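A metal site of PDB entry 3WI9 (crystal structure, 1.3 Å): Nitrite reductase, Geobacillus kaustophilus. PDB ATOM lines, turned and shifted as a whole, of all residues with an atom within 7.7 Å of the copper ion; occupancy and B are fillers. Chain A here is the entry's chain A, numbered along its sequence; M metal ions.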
ATOM      1  N   ALA A  48     -17.095 -22.174 -33.197  1.00  0.00           N
ATOM      2  CA  ALA A  48     -17.408 -20.754 -33.069  1.00  0.00           C
ATOM      3  C   ALA A  48     -16.252 -20.009 -33.712  1.00  0.00           C
ATOM      4  O   ALA A  48     -15.087 -20.283 -33.406  1.00  0.00           O
ATOM      5  CB  ALA A  48     -17.554 -20.374 -31.606  1.00  0.00           C
ATOM      6  N   TRP A  64     -20.032 -12.917 -35.699  1.00  0.00           N
ATOM      7  CA  TRP A  64     -19.735 -13.999 -34.775  1.00  0.00           C
ATOM      8  C   TRP A  64     -20.607 -15.155 -35.252  1.00  0.00           C
ATOM      9  O   TRP A  64     -21.831 -15.014 -35.385  1.00  0.00           O
ATOM     10  CB  TRP A  64     -20.112 -13.622 -33.344  1.00  0.00           C
ATOM     11  CG  TRP A  64     -19.402 -12.433 -32.747  1.00  0.00           C
ATOM     12  CD1 TRP A  64     -18.569 -11.546 -33.367  1.00  0.00           C
ATOM     13  CD2 TRP A  64     -19.519 -12.009 -31.394  1.00  0.00           C
ATOM     14  NE1 TRP A  64     -18.141 -10.594 -32.466  1.00  0.00           N
ATOM     15  CE2 TRP A  64     -18.713 -10.850 -31.246  1.00  0.00           C
ATOM     16  CE3 TRP A  64     -20.238 -12.478 -30.296  1.00  0.00           C
ATOM     17  CZ2 TRP A  64     -18.604 -10.173 -30.025  1.00  0.00           C
ATOM     18  CZ3 TRP A  64     -20.126 -11.824 -29.093  1.00  0.00           C
ATOM     19  CH2 TRP A  64     -19.322 -10.676 -28.964  1.00  0.00           C
ATOM     20  N   THR A  65     -19.979 -16.303 -35.527  1.00  0.00           N
ATOM     21  CA  THR A  65     -20.682 -17.378 -36.224  1.00  0.00           C
ATOM     22  C   THR A  65     -20.411 -18.759 -35.649  1.00  0.00           C
ATOM     23  O   THR A  65     -19.422 -18.976 -34.942  1.00  0.00           O
ATOM     24  CB  THR A  65     -20.249 -17.449 -37.730  1.00  0.00           C
ATOM     25  OG1 THR A  65     -18.929 -18.011 -37.812  1.00  0.00           O
ATOM     26  CG2 THR A  65     -20.247 -16.063 -38.398  1.00  0.00           C
ATOM     27  N   PHE A  66     -21.310 -19.684 -35.975  1.00  0.00           N
ATOM     28  CA  PHE A  66     -20.979 -21.094 -35.999  1.00  0.00           C
ATOM     29  C   PHE A  66     -20.509 -21.467 -37.413  1.00  0.00           C
ATOM     30  O   PHE A  66     -21.220 -21.266 -38.394  1.00  0.00           O
ATOM     31  CB  PHE A  66     -22.178 -21.957 -35.579  1.00  0.00           C
ATOM     32  CG  PHE A  66     -22.651 -21.698 -34.187  1.00  0.00           C
ATOM     33  CD1 PHE A  66     -21.949 -22.187 -33.083  1.00  0.00           C
ATOM     34  CD2 PHE A  66     -23.831 -21.002 -33.957  1.00  0.00           C
ATOM     35  CE1 PHE A  66     -22.397 -21.962 -31.785  1.00  0.00           C
ATOM     36  CE2 PHE A  66     -24.293 -20.757 -32.654  1.00  0.00           C
ATOM     37  CZ  PHE A  66     -23.587 -21.248 -31.569  1.00  0.00           C
ATOM     38  N   LEU A  87     -18.242 -28.333 -29.470  1.00  0.00           N
ATOM     39  CA  LEU A  87     -17.969 -26.983 -29.964  1.00  0.00           C
ATOM     40  C   LEU A  87     -16.491 -26.647 -29.812  1.00  0.00           C
ATOM     41  O   LEU A  87     -15.956 -26.691 -28.691  1.00  0.00           O
ATOM     42  CB  LEU A  87     -18.807 -25.946 -29.209  1.00  0.00           C
ATOM     43  CG  LEU A  87     -18.664 -24.486 -29.684  1.00  0.00           C
ATOM     44  CD1 LEU A  87     -19.248 -24.335 -31.087  1.00  0.00           C
ATOM     45  CD2 LEU A  87     -19.343 -23.537 -28.709  1.00  0.00           C
ATOM     46  N   ASN A  89     -14.039 -23.614 -30.039  1.00  0.00           N
ATOM     47  CA  ASN A  89     -14.040 -22.151 -30.082  1.00  0.00           C
ATOM     48  C   ASN A  89     -12.762 -21.595 -30.708  1.00  0.00           C
ATOM     49  O   ASN A  89     -11.689 -21.672 -30.108  1.00  0.00           O
ATOM     50  CB  ASN A  89     -14.263 -21.551 -28.691  1.00  0.00           C
ATOM     51  CG  ASN A  89     -14.458 -20.056 -28.731  1.00  0.00           C
ATOM     52  OD1 ASN A  89     -14.535 -19.482 -29.810  1.00  0.00           O
ATOM     53  ND2 ASN A  89     -14.535 -19.418 -27.572  1.00  0.00           N
ATOM     54  N   ASP A  91     -12.586 -18.330 -31.726  1.00  0.00           N
ATOM     55  CA  ASP A  91     -12.509 -16.925 -31.373  1.00  0.00           C
ATOM     56  C   ASP A  91     -11.307 -16.716 -30.446  1.00  0.00           C
ATOM     57  O   ASP A  91     -11.213 -17.381 -29.418  1.00  0.00           O
ATOM     58  CB  ASP A  91     -13.810 -16.508 -30.664  1.00  0.00           C
ATOM     59  CG  ASP A  91     -13.955 -15.013 -30.511  1.00  0.00           C
ATOM     60  OD1 ASP A  91     -12.940 -14.317 -30.248  1.00  0.00           O
ATOM     61  OD2 ASP A  91     -15.096 -14.539 -30.614  1.00  0.00           O
ATOM     62  N   VAL A  94     -13.235 -14.198 -27.201  1.00  0.00           N
ATOM     63  CA  VAL A  94     -14.588 -14.292 -26.605  1.00  0.00           C
ATOM     64  C   VAL A  94     -15.009 -15.744 -26.395  1.00  0.00           C
ATOM     65  O   VAL A  94     -14.912 -16.539 -27.325  1.00  0.00           O
ATOM     66  CB  VAL A  94     -15.674 -13.574 -27.451  1.00  0.00           C
ATOM     67  CG1 VAL A  94     -16.972 -13.439 -26.658  1.00  0.00           C
ATOM     68  CG2 VAL A  94     -15.189 -12.199 -27.877  1.00  0.00           C
ATOM     69  N   PRO A  95     -15.482 -16.093 -25.180  1.00  0.00           N
ATOM     70  CA  PRO A  95     -16.073 -17.422 -25.001  1.00  0.00           C
ATOM     71  C   PRO A  95     -17.382 -17.572 -25.778  1.00  0.00           C
ATOM     72  O   PRO A  95     -18.090 -16.582 -26.026  1.00  0.00           O
ATOM     73  CB  PRO A  95     -16.363 -17.492 -23.499  1.00  0.00           C
ATOM     74  CG  PRO A  95     -15.538 -16.381 -22.884  1.00  0.00           C
ATOM     75  CD  PRO A  95     -15.478 -15.320 -23.924  1.00  0.00           C
ATOM     76  N   HIS A  96     -17.693 -18.804 -26.157  1.00  0.00           N
ATOM     77  CA  HIS A  96     -18.953 -19.101 -26.853  1.00  0.00           C
ATOM     78  C   HIS A  96     -19.561 -20.417 -26.362  1.00  0.00           C
ATOM     79  O   HIS A  96     -18.893 -21.210 -25.689  1.00  0.00           O
ATOM     80  CB  HIS A  96     -18.754 -19.116 -28.386  1.00  0.00           C
ATOM     81  CG  HIS A  96     -18.286 -17.797 -28.934  1.00  0.00           C
ATOM     82  ND1 HIS A  96     -19.116 -16.695 -29.028  1.00  0.00           N
ATOM     83  CD2 HIS A  96     -17.087 -17.407 -29.438  1.00  0.00           C
ATOM     84  CE1 HIS A  96     -18.431 -15.678 -29.543  1.00  0.00           C
ATOM     85  NE2 HIS A  96     -17.197 -16.092 -29.796  1.00  0.00           N
ATOM     86  N   SER A  97     -20.838 -20.634 -26.670  1.00  0.00           N
ATOM     87  CA  SER A  97     -21.556 -21.804 -26.200  1.00  0.00           C
ATOM     88  C   SER A  97     -22.633 -22.176 -27.214  1.00  0.00           C
ATOM     89  O   SER A  97     -22.811 -21.486 -28.228  1.00  0.00           O
ATOM     90  CB  SER A  97     -22.231 -21.506 -24.858  1.00  0.00           C
ATOM     91  OG  SER A  97     -23.081 -20.367 -24.980  1.00  0.00           O
ATOM     92  N   MET A  98     -23.341 -23.265 -26.942  1.00  0.00           N
ATOM     93  CA  MET A  98     -24.437 -23.723 -27.789  1.00  0.00           C
ATOM     94  C   MET A  98     -25.676 -24.087 -26.988  1.00  0.00           C
ATOM     95  O   MET A  98     -25.600 -24.843 -26.018  1.00  0.00           O
ATOM     96  CB  MET A  98     -23.991 -24.933 -28.623  1.00  0.00           C
ATOM     97  CG  MET A  98     -25.100 -25.557 -29.480  1.00  0.00           C
ATOM     98  SD  MET A  98     -25.765 -24.425 -30.740  1.00  0.00           S
ATOM     99  CE  MET A  98     -24.583 -24.732 -32.040  1.00  0.00           C
ATOM    100  N   ASP A 113     -20.094 -22.139 -21.340  1.00  0.00           N
ATOM    101  CA  ASP A 113     -19.098 -21.481 -22.178  1.00  0.00           C
ATOM    102  C   ASP A 113     -17.905 -22.380 -22.471  1.00  0.00           C
ATOM    103  O   ASP A 113     -17.514 -23.223 -21.651  1.00  0.00           O
ATOM    104  CB  ASP A 113     -18.629 -20.175 -21.521  1.00  0.00           C
ATOM    105  CG  ASP A 113     -19.712 -19.101 -21.517  1.00  0.00           C
ATOM    106  OD1 ASP A 113     -19.586 -18.130 -20.744  1.00  0.00           O
ATOM    107  OD2 ASP A 113     -20.694 -19.234 -22.277  1.00  0.00           O
ATOM    108  N   HIS A 135     -28.626 -21.434 -30.945  1.00  0.00           N
ATOM    109  CA  HIS A 135     -27.899 -20.159 -30.820  1.00  0.00           C
ATOM    110  C   HIS A 135     -26.876 -20.246 -29.719  1.00  0.00           C
ATOM    111  O   HIS A 135     -26.954 -21.118 -28.839  1.00  0.00           O
ATOM    112  CB  HIS A 135     -28.846 -18.963 -30.576  1.00  0.00           C
ATOM    113  CG  HIS A 135     -29.674 -19.082 -29.332  1.00  0.00           C
ATOM    114  ND1 HIS A 135     -29.218 -18.690 -28.086  1.00  0.00           N
ATOM    115  CD2 HIS A 135     -30.931 -19.569 -29.136  1.00  0.00           C
ATOM    116  CE1 HIS A 135     -30.158 -18.907 -27.180  1.00  0.00           C
ATOM    117  NE2 HIS A 135     -31.204 -19.448 -27.788  1.00  0.00           N
ATOM    118  N   CYS A 136     -25.920 -19.331 -29.769  1.00  0.00           N
ATOM    119  CA  CYS A 136     -24.973 -19.164 -28.661  1.00  0.00           C
ATOM    120  C   CYS A 136     -25.702 -18.705 -27.392  1.00  0.00           C
ATOM    121  O   CYS A 136     -26.622 -17.886 -27.461  1.00  0.00           O
ATOM    122  CB  CYS A 136     -23.884 -18.179 -29.059  1.00  0.00           C
ATOM    123  SG  CYS A 136     -22.664 -17.864 -27.780  1.00  0.00           S
ATOM    124  N   GLY A 137     -25.337 -19.288 -26.250  1.00  0.00           N
ATOM    125  CA  GLY A 137     -25.979 -18.960 -24.976  1.00  0.00           C
ATOM    126  C   GLY A 137     -25.088 -18.200 -24.006  1.00  0.00           C
ATOM    127  O   GLY A 137     -25.309 -18.244 -22.789  1.00  0.00           O
ATOM    128  N   THR A 138     -24.097 -17.490 -24.533  1.00  0.00           N
ATOM    129  CA  THR A 138     -23.129 -16.759 -23.710  1.00  0.00           C
ATOM    130  C   THR A 138     -23.612 -15.349 -23.388  1.00  0.00           C
ATOM    131  O   THR A 138     -24.071 -14.626 -24.273  1.00  0.00           O
ATOM    132  CB  THR A 138     -21.733 -16.768 -24.403  1.00  0.00           C
ATOM    133  OG1 THR A 138     -21.314 -18.132 -24.587  1.00  0.00           O
ATOM    134  CG2 THR A 138     -20.678 -16.030 -23.585  1.00  0.00           C
ATOM    135  N   LYS A 139     -23.487 -14.949 -22.122  1.00  0.00           N
ATOM    136  CA  LYS A 139     -23.883 -13.606 -21.677  1.00  0.00           C
ATOM    137  C   LYS A 139     -22.978 -12.530 -22.279  1.00  0.00           C
ATOM    138  O   LYS A 139     -21.749 -12.693 -22.277  1.00  0.00           O
ATOM    139  CB  LYS A 139     -23.824 -13.534 -20.143  1.00  0.00           C
ATOM    140  CG  LYS A 139     -24.105 -12.146 -19.569  1.00  0.00           C
ATOM    141  CD  LYS A 139     -24.092 -12.151 -18.036  1.00  0.00           C
ATOM    142  CE  LYS A 139     -24.597 -10.816 -17.499  1.00  0.00           C
ATOM    143  NZ  LYS A 139     -24.599 -10.742 -16.006  1.00  0.00           N
ATOM    144  N   PRO A 140     -23.562 -11.443 -22.817  1.00  0.00           N
ATOM    145  CA  PRO A 140     -24.984 -11.149 -23.038  1.00  0.00           C
ATOM    146  C   PRO A 140     -25.509 -11.919 -24.237  1.00  0.00           C
ATOM    147  O   PRO A 140     -24.963 -11.779 -25.330  1.00  0.00           O
ATOM    148  CB  PRO A 140     -25.002  -9.634 -23.333  1.00  0.00           C
ATOM    149  CG  PRO A 140     -23.615  -9.133 -23.028  1.00  0.00           C
ATOM    150  CD  PRO A 140     -22.713 -10.305 -23.220  1.00  0.00           C
ATOM    151  N   VAL A 141     -26.537 -12.737 -24.034  1.00  0.00           N
ATOM    152  CA  VAL A 141     -27.052 -13.587 -25.122  1.00  0.00           C
ATOM    153  C   VAL A 141     -27.480 -12.734 -26.327  1.00  0.00           C
ATOM    154  O   VAL A 141     -27.185 -13.082 -27.480  1.00  0.00           O
ATOM    155  CB  VAL A 141     -28.162 -14.528 -24.619  1.00  0.00           C
ATOM    156  CG1 VAL A 141     -28.800 -15.327 -25.764  1.00  0.00           C
ATOM    157  CG2 VAL A 141     -27.601 -15.490 -23.555  1.00  0.00           C
ATOM    158  N   GLN A 143     -26.125 -10.052 -27.431  1.00  0.00           N
ATOM    159  CA  GLN A 143     -24.938  -9.705 -28.200  1.00  0.00           C
ATOM    160  C   GLN A 143     -24.493 -10.856 -29.089  1.00  0.00           C
ATOM    161  O   GLN A 143     -24.205 -10.653 -30.286  1.00  0.00           O
ATOM    162  CB  GLN A 143     -23.821  -9.273 -27.255  1.00  0.00           C
ATOM    163  CG  GLN A 143     -22.578  -8.787 -27.963  1.00  0.00           C
ATOM    164  CD  GLN A 143     -21.549  -8.235 -26.992  1.00  0.00           C
ATOM    165  OE1 GLN A 143     -21.545  -8.573 -25.813  1.00  0.00           O
ATOM    166  NE2 GLN A 143     -20.658  -7.386 -27.497  1.00  0.00           N
ATOM    167  N   HIS A 144     -24.484 -12.071 -28.544  1.00  0.00           N
ATOM    168  CA  HIS A 144     -24.021 -13.224 -29.307  1.00  0.00           C
ATOM    169  C   HIS A 144     -24.984 -13.589 -30.443  1.00  0.00           C
ATOM    170  O   HIS A 144     -24.533 -13.856 -31.554  1.00  0.00           O
ATOM    171  CB  HIS A 144     -23.723 -14.410 -28.396  1.00  0.00           C
ATOM    172  CG  HIS A 144     -22.508 -14.207 -27.537  1.00  0.00           C
ATOM    173  ND1 HIS A 144     -21.315 -14.876 -27.757  1.00  0.00           N
ATOM    174  CD2 HIS A 144     -22.296 -13.400 -26.481  1.00  0.00           C
ATOM    175  CE1 HIS A 144     -20.430 -14.493 -26.850  1.00  0.00           C
ATOM    176  NE2 HIS A 144     -20.993 -13.583 -26.076  1.00  0.00           N
ATOM    177  N   ILE A 145     -26.283 -13.520 -30.176  1.00  0.00           N
ATOM    178  CA  ILE A 145     -27.249 -13.759 -31.231  1.00  0.00           C
ATOM    179  C   ILE A 145     -27.182 -12.655 -32.294  1.00  0.00           C
ATOM    180  O   ILE A 145     -27.086 -12.955 -33.487  1.00  0.00           O
ATOM    181  CB  ILE A 145     -28.706 -13.918 -30.710  1.00  0.00           C
ATOM    182  CG1 ILE A 145     -28.831 -15.157 -29.800  1.00  0.00           C
ATOM    183  CG2 ILE A 145     -29.654 -14.000 -31.906  1.00  0.00           C
ATOM    184  CD1 ILE A 145     -30.187 -15.300 -29.109  1.00  0.00           C
ATOM    185  N   ASN A 147     -24.916 -10.663 -33.208  1.00  0.00           N
ATOM    186  CA  ASN A 147     -23.701 -10.702 -34.013  1.00  0.00           C
ATOM    187  C   ASN A 147     -23.628 -11.863 -35.010  1.00  0.00           C
ATOM    188  O   ASN A 147     -22.712 -11.912 -35.828  1.00  0.00           O
ATOM    189  CB  ASN A 147     -22.437 -10.632 -33.146  1.00  0.00           C
ATOM    190  CG  ASN A 147     -22.126  -9.218 -32.659  1.00  0.00           C
ATOM    191  OD1 ASN A 147     -22.366  -8.234 -33.360  1.00  0.00           O
ATOM    192  ND2 ASN A 147     -21.551  -9.125 -31.460  1.00  0.00           N
ATOM    193  N   MET A 149     -24.757 -15.493 -34.138  1.00  0.00           N
ATOM    194  CA  MET A 149     -24.707 -16.871 -33.624  1.00  0.00           C
ATOM    195  C   MET A 149     -26.080 -17.510 -33.417  1.00  0.00           C
ATOM    196  O   MET A 149     -26.551 -17.684 -32.276  1.00  0.00           O
ATOM    197  CB  MET A 149     -23.857 -16.964 -32.350  1.00  0.00           C
ATOM    198  CG  MET A 149     -22.503 -16.291 -32.543  1.00  0.00           C
ATOM    199  SD  MET A 149     -21.246 -16.691 -31.303  1.00  0.00           S
ATOM    200  CE  MET A 149     -20.906 -18.409 -31.699  1.00  0.00           C
HETATM  201 CU    CU M   1     -21.154 -16.670 -28.699  1.00  0.00          CU
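Four residues have an atom within 4 Å of the copper ion: His 96, Cys 136, His 144 and Met 149.
A ring nitrogen (NE2) of His 96 lies close to the backbone carbonyl oxygen (O) of Val 94. OD2 of Asp 91 is in hydrogen-bond range of NE2 of His 96 (2.7 Å). The side-chain sulfur (SG) of Cys 136 lies close to the side-chain hydroxyl (OG1) of Thr 138 (3.5 Å). The side-chain sulfur (SG) of Cys 136 sits close to the backbone NH (N) of Ser 97 (3.5 Å). The backbone NH (N) of Met 149 lies close to the backbone carbonyl oxygen (O) of Trp 64 (3.2 Å).
The copper ion is bound by ND1 of His 144 (2.0 Å), ND1 of His 96 (2.1 Å), SG of Cys 136 (2.1 Å) and SD of Met 149 (2.6 Å). The copper ion has four donor atoms within binding distance.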
